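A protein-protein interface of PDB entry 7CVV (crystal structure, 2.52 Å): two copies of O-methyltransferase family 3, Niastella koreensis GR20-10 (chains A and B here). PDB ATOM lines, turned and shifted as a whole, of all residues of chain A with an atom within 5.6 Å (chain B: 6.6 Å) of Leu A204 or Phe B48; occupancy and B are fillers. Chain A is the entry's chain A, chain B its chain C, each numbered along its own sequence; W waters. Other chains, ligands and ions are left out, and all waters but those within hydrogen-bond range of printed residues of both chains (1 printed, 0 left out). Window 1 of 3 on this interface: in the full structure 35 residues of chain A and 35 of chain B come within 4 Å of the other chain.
Phe A48 touches Leu B204, and with the chains exchanged Leu A204 touches Phe B48. Phe A48 touches Leu B217, and with the chains exchanged Leu A217 touches Phe B48. Of the 8 pairs that touch across the chains among the printed residues, 4 have their exchanged pair printed and touching as well.
Hydrophobic or aromatic side chains of chain B within 4 Å of the printed part of chain A: Ile B13, Phe B48, Leu B51, Leu B204 and Leu B217. Along chain B the printed residues that touch a printed residue of chain A span positions 13 to 217. Of the 12 printed residues of chain A, 5 touch a printed residue of chain B. Hydrophobic or aromatic side chains of chain A within 4 Å of the printed part of chain B: Phe A48, Leu A204 and Leu A217. Among the printed residues, no Asp or Glu carboxylate lies within 4 Å of a Lys or Arg side-chain nitrogen of the other chain.
N of Leu B204 sits at hydrogen-bond distance from O of Met B215 (2.9 Å). O of Thr A202 sits at hydrogen-bond distance from N of Leu A217. N of Leu A204 is in hydrogen-bond range of O of Met A215, at 2.7 Å.
Among the printed residues, pairs that only touch across the chains: Thr A202 with Leu B51 (3.6 Å), Ile A203 with Ile B13 (3.6 Å), Leu A217 with Phe B48 (3.7 Å), Phe A48 with Leu B217 (3.7 Å), Thr A202 with Lys B47 (3.8 Å), Leu A204 with Phe B48 (3.8 Å), Phe A48 with Leu B204 (3.9 Å) and Thr A202 with Asn B44 (3.9 Å).
Of the printed residues of chain B, Phe A48 touches Leu B204 and Leu B217. Printed residues of chain B within 4 Å of Ile A203: Ile B13. Leu A204 touches just one residue of chain B: Phe B48. Gln A205 touches none of the printed residues of chain B. Of the printed residues of chain A, Ile B13 touches Ile A203. Of chain A, only Leu A204 and Leu A217 come within 4 Å of Phe B48. Met B135 touches none of the printed residues of chain A. Printed residues of chain A within 4 Å of Leu B217: Phe A48 (3.7 Å). The nearest residue of chain B that does not touch Leu A204 is Leu B204 (4.04 Å). The nearest printed residue of chain A that does not touch Phe B48 is Thr A202 (4.1 Å).
Water W1 lies within hydrogen-bond range of OG1 of Thr A202 (2.6 Å) and OD1 of Asn B44 (2.7 Å).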
ATOM      1  N   PHE A  48      20.923 -31.148  -0.554  1.00  0.00           N
ATOM      2  CA  PHE A  48      21.209 -29.837  -1.194  1.00  0.00           C
ATOM      3  C   PHE A  48      20.252 -28.770  -0.634  1.00  0.00           C
ATOM      4  O   PHE A  48      20.691 -27.682  -0.221  1.00  0.00           O
ATOM      5  CB  PHE A  48      21.140 -29.968  -2.713  1.00  0.00           C
ATOM      6  CG  PHE A  48      21.536 -28.708  -3.431  1.00  0.00           C
ATOM      7  CD1 PHE A  48      22.571 -27.920  -2.959  1.00  0.00           C
ATOM      8  CD2 PHE A  48      20.870 -28.302  -4.581  1.00  0.00           C
ATOM      9  CE1 PHE A  48      22.936 -26.766  -3.635  1.00  0.00           C
ATOM     10  CE2 PHE A  48      21.255 -27.155  -5.265  1.00  0.00           C
ATOM     11  CZ  PHE A  48      22.288 -26.395  -4.792  1.00  0.00           C
ATOM     12  N   ILE A 168      13.240 -27.588 -16.394  1.00  0.00           N
ATOM     13  CA  ILE A 168      13.962 -28.013 -17.637  1.00  0.00           C
ATOM     14  C   ILE A 168      13.163 -29.118 -18.355  1.00  0.00           C
ATOM     15  O   ILE A 168      13.028 -29.047 -19.601  1.00  0.00           O
ATOM     16  CB  ILE A 168      15.389 -28.462 -17.267  1.00  0.00           C
ATOM     17  CG1 ILE A 168      16.299 -27.265 -16.957  1.00  0.00           C
ATOM     18  CG2 ILE A 168      15.986 -29.361 -18.339  1.00  0.00           C
ATOM     19  CD1 ILE A 168      16.415 -26.237 -18.061  1.00  0.00           C
ATOM     20  N   THR A 202      19.890 -18.211 -11.599  1.00  0.00           N
ATOM     21  CA  THR A 202      20.406 -19.202 -12.568  1.00  0.00           C
ATOM     22  C   THR A 202      19.480 -20.423 -12.526  1.00  0.00           C
ATOM     23  O   THR A 202      18.525 -20.460 -11.696  1.00  0.00           O
ATOM     24  CB  THR A 202      21.883 -19.467 -12.266  1.00  0.00           C
ATOM     25  OG1 THR A 202      22.497 -19.982 -13.449  1.00  0.00           O
ATOM     26  CG2 THR A 202      22.078 -20.394 -11.087  1.00  0.00           C
ATOM     27  N   ILE A 203      19.715 -21.367 -13.430  1.00  0.00           N
ATOM     28  CA  ILE A 203      19.082 -22.710 -13.396  1.00  0.00           C
ATOM     29  C   ILE A 203      20.190 -23.757 -13.403  1.00  0.00           C
ATOM     30  O   ILE A 203      21.015 -23.696 -14.347  1.00  0.00           O
ATOM     31  CB  ILE A 203      18.133 -22.890 -14.586  1.00  0.00           C
ATOM     32  CG1 ILE A 203      17.038 -21.812 -14.600  1.00  0.00           C
ATOM     33  CG2 ILE A 203      17.581 -24.305 -14.576  1.00  0.00           C
ATOM     34  CD1 ILE A 203      16.323 -21.628 -15.938  1.00  0.00           C
ATOM     35  N   LEU A 204      20.176 -24.664 -12.414  1.00  0.00           N
ATOM     36  CA  LEU A 204      21.061 -25.862 -12.336  1.00  0.00           C
ATOM     37  C   LEU A 204      20.476 -27.043 -13.109  1.00  0.00           C
ATOM     38  O   LEU A 204      19.361 -27.474 -12.812  1.00  0.00           O
ATOM     39  CB  LEU A 204      21.240 -26.306 -10.882  1.00  0.00           C
ATOM     40  CG  LEU A 204      21.922 -25.314  -9.958  1.00  0.00           C
ATOM     41  CD1 LEU A 204      22.069 -25.925  -8.573  1.00  0.00           C
ATOM     42  CD2 LEU A 204      23.268 -24.882 -10.523  1.00  0.00           C
ATOM     43  N   GLN A 205      21.283 -27.628 -13.980  1.00  0.00           N
ATOM     44  CA  GLN A 205      21.024 -28.945 -14.602  1.00  0.00           C
ATOM     45  C   GLN A 205      21.430 -30.048 -13.626  1.00  0.00           C
ATOM     46  O   GLN A 205      22.598 -30.063 -13.215  1.00  0.00           O
ATOM     47  CB  GLN A 205      21.808 -29.016 -15.902  1.00  0.00           C
ATOM     48  CG  GLN A 205      21.062 -28.371 -17.052  1.00  0.00           C
ATOM     49  CD  GLN A 205      21.853 -28.535 -18.319  1.00  0.00           C
ATOM     50  OE1 GLN A 205      22.768 -27.754 -18.597  1.00  0.00           O
ATOM     51  NE2 GLN A 205      21.497 -29.546 -19.094  1.00  0.00           N
ATOM     52  N   MET A 206      20.510 -30.935 -13.271  1.00  0.00           N
ATOM     53  CA  MET A 206      20.766 -32.018 -12.297  1.00  0.00           C
ATOM     54  C   MET A 206      20.659 -33.378 -12.976  1.00  0.00           C
ATOM     55  O   MET A 206      19.744 -33.567 -13.778  1.00  0.00           O
ATOM     56  CB  MET A 206      19.759 -31.942 -11.159  1.00  0.00           C
ATOM     57  CG  MET A 206      19.711 -30.563 -10.569  1.00  0.00           C
ATOM     58  SD  MET A 206      19.181 -30.563  -8.862  1.00  0.00           S
ATOM     59  CE  MET A 206      17.474 -31.070  -9.076  1.00  0.00           C
ATOM     60  N   ASP A 213      16.724 -33.178 -14.763  1.00  0.00           N
ATOM     61  CA  ASP A 213      15.940 -32.312 -13.845  1.00  0.00           C
ATOM     62  C   ASP A 213      16.569 -30.925 -14.013  1.00  0.00           C
ATOM     63  O   ASP A 213      17.744 -30.850 -14.431  1.00  0.00           O
ATOM     64  CB  ASP A 213      16.042 -32.895 -12.418  1.00  0.00           C
ATOM     65  CG  ASP A 213      15.046 -32.468 -11.333  1.00  0.00           C
ATOM     66  OD1 ASP A 213      14.851 -31.243 -11.148  1.00  0.00           O
ATOM     67  OD2 ASP A 213      14.521 -33.380 -10.613  1.00  0.00           O
ATOM     68  N   GLY A 214      15.830 -29.859 -13.748  1.00  0.00           N
ATOM     69  CA  GLY A 214      16.417 -28.516 -13.673  1.00  0.00           C
ATOM     70  C   GLY A 214      15.870 -27.815 -12.467  1.00  0.00           C
ATOM     71  O   GLY A 214      14.637 -27.814 -12.317  1.00  0.00           O
ATOM     72  N   MET A 215      16.743 -27.253 -11.637  1.00  0.00           N
ATOM     73  CA  MET A 215      16.331 -26.437 -10.472  1.00  0.00           C
ATOM     74  C   MET A 215      16.652 -24.957 -10.726  1.00  0.00           C
ATOM     75  O   MET A 215      17.795 -24.663 -11.126  1.00  0.00           O
ATOM     76  CB  MET A 215      17.058 -26.914  -9.221  1.00  0.00           C
ATOM     77  CG  MET A 215      16.137 -27.044  -8.066  1.00  0.00           C
ATOM     78  SD  MET A 215      17.053 -27.623  -6.633  1.00  0.00           S
ATOM     79  CE  MET A 215      15.996 -28.964  -6.076  1.00  0.00           C
ATOM     80  N   ALA A 216      15.695 -24.057 -10.495  1.00  0.00           N
ATOM     81  CA  ALA A 216      15.913 -22.591 -10.545  1.00  0.00           C
ATOM     82  C   ALA A 216      16.306 -22.106  -9.148  1.00  0.00           C
ATOM     83  O   ALA A 216      15.649 -22.504  -8.172  1.00  0.00           O
ATOM     84  CB  ALA A 216      14.678 -21.863 -11.034  1.00  0.00           C
ATOM     85  N   LEU A 217      17.343 -21.278  -9.060  1.00  0.00           N
ATOM     86  CA  LEU A 217      17.733 -20.553  -7.823  1.00  0.00           C
ATOM     87  C   LEU A 217      17.670 -19.047  -8.088  1.00  0.00           C
ATOM     88  O   LEU A 217      18.295 -18.588  -9.052  1.00  0.00           O
ATOM     89  CB  LEU A 217      19.144 -20.987  -7.438  1.00  0.00           C
ATOM     90  CG  LEU A 217      19.338 -22.502  -7.394  1.00  0.00           C
ATOM     91  CD1 LEU A 217      20.736 -22.854  -6.905  1.00  0.00           C
ATOM     92  CD2 LEU A 217      18.283 -23.139  -6.509  1.00  0.00           C
ATOM     93  N   ILE B  13      19.870 -21.699 -20.931  1.00  0.00           N
ATOM     94  CA  ILE B  13      20.020 -21.112 -19.572  1.00  0.00           C
ATOM     95  C   ILE B  13      20.888 -19.851 -19.670  1.00  0.00           C
ATOM     96  O   ILE B  13      20.483 -18.837 -19.055  1.00  0.00           O
ATOM     97  CB  ILE B  13      20.552 -22.147 -18.558  1.00  0.00           C
ATOM     98  CG1 ILE B  13      19.536 -23.266 -18.329  1.00  0.00           C
ATOM     99  CG2 ILE B  13      20.919 -21.467 -17.251  1.00  0.00           C
ATOM    100  CD1 ILE B  13      20.142 -24.531 -17.748  1.00  0.00           C
ATOM    101  N   PRO B  43      29.856 -19.959 -18.113  1.00  0.00           N
ATOM    102  CA  PRO B  43      29.111 -18.776 -17.680  1.00  0.00           C
ATOM    103  C   PRO B  43      28.108 -19.150 -16.576  1.00  0.00           C
ATOM    104  O   PRO B  43      27.988 -18.434 -15.613  1.00  0.00           O
ATOM    105  CB  PRO B  43      28.375 -18.313 -18.952  1.00  0.00           C
ATOM    106  CG  PRO B  43      29.183 -18.888 -20.098  1.00  0.00           C
ATOM    107  CD  PRO B  43      29.812 -20.161 -19.569  1.00  0.00           C
ATOM    108  N   ASN B  44      27.403 -20.268 -16.757  1.00  0.00           N
ATOM    109  CA  ASN B  44      26.311 -20.718 -15.864  1.00  0.00           C
ATOM    110  C   ASN B  44      26.898 -21.110 -14.504  1.00  0.00           C
ATOM    111  O   ASN B  44      26.319 -20.709 -13.477  1.00  0.00           O
ATOM    112  CB  ASN B  44      25.457 -21.775 -16.559  1.00  0.00           C
ATOM    113  CG  ASN B  44      24.579 -21.126 -17.604  1.00  0.00           C
ATOM    114  OD1 ASN B  44      24.360 -19.918 -17.553  1.00  0.00           O
ATOM    115  ND2 ASN B  44      24.082 -21.903 -18.553  1.00  0.00           N
ATOM    116  N   GLN B  45      28.051 -21.764 -14.462  1.00  0.00           N
ATOM    117  CA  GLN B  45      28.726 -22.021 -13.163  1.00  0.00           C
ATOM    118  C   GLN B  45      29.174 -20.691 -12.565  1.00  0.00           C
ATOM    119  O   GLN B  45      29.005 -20.515 -11.341  1.00  0.00           O
ATOM    120  CB  GLN B  45      29.891 -22.985 -13.334  1.00  0.00           C
ATOM    121  CG  GLN B  45      29.458 -24.374 -13.772  1.00  0.00           C
ATOM    122  CD  GLN B  45      30.661 -25.250 -13.999  1.00  0.00           C
ATOM    123  OE1 GLN B  45      31.523 -25.390 -13.122  1.00  0.00           O
ATOM    124  NE2 GLN B  45      30.737 -25.822 -15.186  1.00  0.00           N
ATOM    125  N   GLY B  46      29.685 -19.779 -13.402  1.00  0.00           N
ATOM    126  CA  GLY B  46      30.040 -18.406 -13.000  1.00  0.00           C
ATOM    127  C   GLY B  46      28.901 -17.764 -12.243  1.00  0.00           C
ATOM    128  O   GLY B  46      29.106 -17.313 -11.086  1.00  0.00           O
ATOM    129  N   LYS B  47      27.712 -17.773 -12.846  1.00  0.00           N
ATOM    130  CA  LYS B  47      26.505 -17.154 -12.244  1.00  0.00           C
ATOM    131  C   LYS B  47      26.143 -17.884 -10.951  1.00  0.00           C
ATOM    132  O   LYS B  47      25.814 -17.222  -9.971  1.00  0.00           O
ATOM    133  CB  LYS B  47      25.325 -17.207 -13.208  1.00  0.00           C
ATOM    134  CG  LYS B  47      24.093 -16.456 -12.731  1.00  0.00           C
ATOM    135  CD  LYS B  47      24.282 -14.957 -12.743  1.00  0.00           C
ATOM    136  CE  LYS B  47      22.999 -14.205 -12.467  1.00  0.00           C
ATOM    137  NZ  LYS B  47      22.064 -14.254 -13.621  1.00  0.00           N
ATOM    138  N   PHE B  48      26.230 -19.209 -10.932  1.00  0.00           N
ATOM    139  CA  PHE B  48      25.893 -20.013  -9.725  1.00  0.00           C
ATOM    140  C   PHE B  48      26.787 -19.582  -8.551  1.00  0.00           C
ATOM    141  O   PHE B  48      26.245 -19.352  -7.449  1.00  0.00           O
ATOM    142  CB  PHE B  48      26.004 -21.507 -10.024  1.00  0.00           C
ATOM    143  CG  PHE B  48      25.667 -22.407  -8.859  1.00  0.00           C
ATOM    144  CD1 PHE B  48      24.716 -22.043  -7.925  1.00  0.00           C
ATOM    145  CD2 PHE B  48      26.313 -23.625  -8.697  1.00  0.00           C
ATOM    146  CE1 PHE B  48      24.404 -22.879  -6.865  1.00  0.00           C
ATOM    147  CE2 PHE B  48      26.009 -24.457  -7.627  1.00  0.00           C
ATOM    148  CZ  PHE B  48      25.040 -24.087  -6.722  1.00  0.00           C
ATOM    149  N   LEU B  49      28.103 -19.439  -8.802  1.00  0.00           N
ATOM    150  CA  LEU B  49      29.148 -19.033  -7.810  1.00  0.00           C
ATOM    151  C   LEU B  49      28.884 -17.614  -7.296  1.00  0.00           C
ATOM    152  O   LEU B  49      29.049 -17.405  -6.071  1.00  0.00           O
ATOM    153  CB  LEU B  49      30.530 -19.099  -8.462  1.00  0.00           C
ATOM    154  CG  LEU B  49      31.058 -20.501  -8.769  1.00  0.00           C
ATOM    155  CD1 LEU B  49      32.280 -20.409  -9.673  1.00  0.00           C
ATOM    156  CD2 LEU B  49      31.379 -21.255  -7.491  1.00  0.00           C
ATOM    157  N   GLN B  50      28.474 -16.700  -8.191  1.00  0.00           N
ATOM    158  CA  GLN B  50      28.075 -15.301  -7.853  1.00  0.00           C
ATOM    159  C   GLN B  50      26.895 -15.309  -6.872  1.00  0.00           C
ATOM    160  O   GLN B  50      26.980 -14.654  -5.854  1.00  0.00           O
ATOM    161  CB  GLN B  50      27.747 -14.518  -9.124  1.00  0.00           C
ATOM    162  CG  GLN B  50      27.576 -13.024  -8.892  1.00  0.00           C
ATOM    163  CD  GLN B  50      27.303 -12.332 -10.201  1.00  0.00           C
ATOM    164  OE1 GLN B  50      26.176 -12.328 -10.691  1.00  0.00           O
ATOM    165  NE2 GLN B  50      28.345 -11.776 -10.797  1.00  0.00           N
ATOM    166  N   LEU B  51      25.854 -16.066  -7.160  1.00  0.00           N
ATOM    167  CA  LEU B  51      24.671 -16.264  -6.282  1.00  0.00           C
ATOM    168  C   LEU B  51      25.086 -16.831  -4.919  1.00  0.00           C
ATOM    169  O   LEU B  51      24.562 -16.369  -3.898  1.00  0.00           O
ATOM    170  CB  LEU B  51      23.710 -17.221  -6.991  1.00  0.00           C
ATOM    171  CG  LEU B  51      22.632 -16.538  -7.823  1.00  0.00           C
ATOM    172  CD1 LEU B  51      22.233 -17.374  -9.029  1.00  0.00           C
ATOM    173  CD2 LEU B  51      21.417 -16.274  -6.962  1.00  0.00           C
ATOM    174  N   LEU B  52      25.944 -17.842  -4.895  1.00  0.00           N
ATOM    175  CA  LEU B  52      26.434 -18.444  -3.627  1.00  0.00           C
ATOM    176  C   LEU B  52      27.146 -17.378  -2.802  1.00  0.00           C
ATOM    177  O   LEU B  52      26.923 -17.323  -1.583  1.00  0.00           O
ATOM    178  CB  LEU B  52      27.387 -19.600  -3.926  1.00  0.00           C
ATOM    179  CG  LEU B  52      26.729 -20.851  -4.488  1.00  0.00           C
ATOM    180  CD1 LEU B  52      27.794 -21.845  -4.915  1.00  0.00           C
ATOM    181  CD2 LEU B  52      25.761 -21.474  -3.487  1.00  0.00           C
ATOM    182  N   ALA B  53      27.955 -16.538  -3.442  1.00  0.00           N
ATOM    183  CA  ALA B  53      28.678 -15.471  -2.727  1.00  0.00           C
ATOM    184  C   ALA B  53      27.665 -14.523  -2.070  1.00  0.00           C
ATOM    185  O   ALA B  53      27.889 -14.168  -0.905  1.00  0.00           O
ATOM    186  CB  ALA B  53      29.654 -14.782  -3.644  1.00  0.00           C
ATOM    187  N   TRP B  74      33.458 -13.103 -11.755  1.00  0.00           N
ATOM    188  CA  TRP B  74      32.033 -13.463 -11.480  1.00  0.00           C
ATOM    189  C   TRP B  74      31.762 -13.219 -10.005  1.00  0.00           C
ATOM    190  O   TRP B  74      30.885 -12.407  -9.688  1.00  0.00           O
ATOM    191  CB  TRP B  74      31.683 -14.911 -11.864  1.00  0.00           C
ATOM    192  CG  TRP B  74      31.202 -15.121 -13.273  1.00  0.00           C
ATOM    193  CD1 TRP B  74      31.904 -15.720 -14.278  1.00  0.00           C
ATOM    194  CD2 TRP B  74      29.905 -14.799 -13.823  1.00  0.00           C
ATOM    195  NE1 TRP B  74      31.139 -15.790 -15.415  1.00  0.00           N
ATOM    196  CE2 TRP B  74      29.910 -15.228 -15.172  1.00  0.00           C
ATOM    197  CE3 TRP B  74      28.754 -14.178 -13.334  1.00  0.00           C
ATOM    198  CZ2 TRP B  74      28.820 -15.036 -16.030  1.00  0.00           C
ATOM    199  CZ3 TRP B  74      27.680 -13.978 -14.182  1.00  0.00           C
ATOM    200  CH2 TRP B  74      27.713 -14.400 -15.514  1.00  0.00           C
ATOM    201  N   MET B 135      33.305 -17.027   1.820  1.00  0.00           N
ATOM    202  CA  MET B 135      33.231 -18.112   0.832  1.00  0.00           C
ATOM    203  C   MET B 135      34.643 -18.438   0.321  1.00  0.00           C
ATOM    204  O   MET B 135      35.437 -17.511   0.039  1.00  0.00           O
ATOM    205  CB  MET B 135      32.318 -17.672  -0.308  1.00  0.00           C
ATOM    206  CG  MET B 135      32.482 -18.476  -1.567  1.00  0.00           C
ATOM    207  SD  MET B 135      31.082 -18.229  -2.659  1.00  0.00           S
ATOM    208  CE  MET B 135      31.580 -19.345  -3.973  1.00  0.00           C
ATOM    209  N   LEU B 204      27.237 -31.851  -6.095  1.00  0.00           N
ATOM    210  CA  LEU B 204      26.338 -31.644  -7.255  1.00  0.00           C
ATOM    211  C   LEU B 204      26.961 -32.272  -8.495  1.00  0.00           C
ATOM    212  O   LEU B 204      28.147 -31.999  -8.783  1.00  0.00           O
ATOM    213  CB  LEU B 204      26.176 -30.146  -7.492  1.00  0.00           C
ATOM    214  CG  LEU B 204      25.318 -29.405  -6.477  1.00  0.00           C
ATOM    215  CD1 LEU B 204      25.144 -27.958  -6.916  1.00  0.00           C
ATOM    216  CD2 LEU B 204      23.962 -30.089  -6.318  1.00  0.00           C
ATOM    217  N   MET B 206      27.235 -31.901 -12.326  1.00  0.00           N
ATOM    218  CA  MET B 206      27.062 -30.782 -13.282  1.00  0.00           C
ATOM    219  C   MET B 206      27.336 -31.246 -14.715  1.00  0.00           C
ATOM    220  O   MET B 206      28.363 -31.945 -14.959  1.00  0.00           O
ATOM    221  CB  MET B 206      28.014 -29.646 -12.930  1.00  0.00           C
ATOM    222  CG  MET B 206      27.856 -29.205 -11.502  1.00  0.00           C
ATOM    223  SD  MET B 206      28.539 -27.562 -11.313  1.00  0.00           S
ATOM    224  CE  MET B 206      30.258 -27.925 -11.677  1.00  0.00           C
ATOM    225  N   MET B 215      30.811 -30.783  -8.171  1.00  0.00           N
ATOM    226  CA  MET B 215      31.166 -29.600  -7.346  1.00  0.00           C
ATOM    227  C   MET B 215      30.759 -29.895  -5.908  1.00  0.00           C
ATOM    228  O   MET B 215      29.563 -30.143  -5.673  1.00  0.00           O
ATOM    229  CB  MET B 215      30.395 -28.377  -7.830  1.00  0.00           C
ATOM    230  CG  MET B 215      30.900 -27.111  -7.263  1.00  0.00           C
ATOM    231  SD  MET B 215      29.997 -25.722  -7.956  1.00  0.00           S
ATOM    232  CE  MET B 215      31.172 -25.199  -9.206  1.00  0.00           C
ATOM    233  N   LEU B 217      30.013 -28.863  -2.023  1.00  0.00           N
ATOM    234  CA  LEU B 217      29.483 -27.713  -1.256  1.00  0.00           C
ATOM    235  C   LEU B 217      29.443 -28.105   0.221  1.00  0.00           C
ATOM    236  O   LEU B 217      28.732 -29.083   0.574  1.00  0.00           O
ATOM    237  CB  LEU B 217      28.090 -27.381  -1.771  1.00  0.00           C
ATOM    238  CG  LEU B 217      28.036 -26.839  -3.193  1.00  0.00           C
ATOM    239  CD1 LEU B 217      26.603 -26.589  -3.595  1.00  0.00           C
ATOM    240  CD2 LEU B 217      28.820 -25.547  -3.304  1.00  0.00           C
HETATM  241  O   HOH W   1      23.034 -18.607 -15.534  1.00  0.00           O
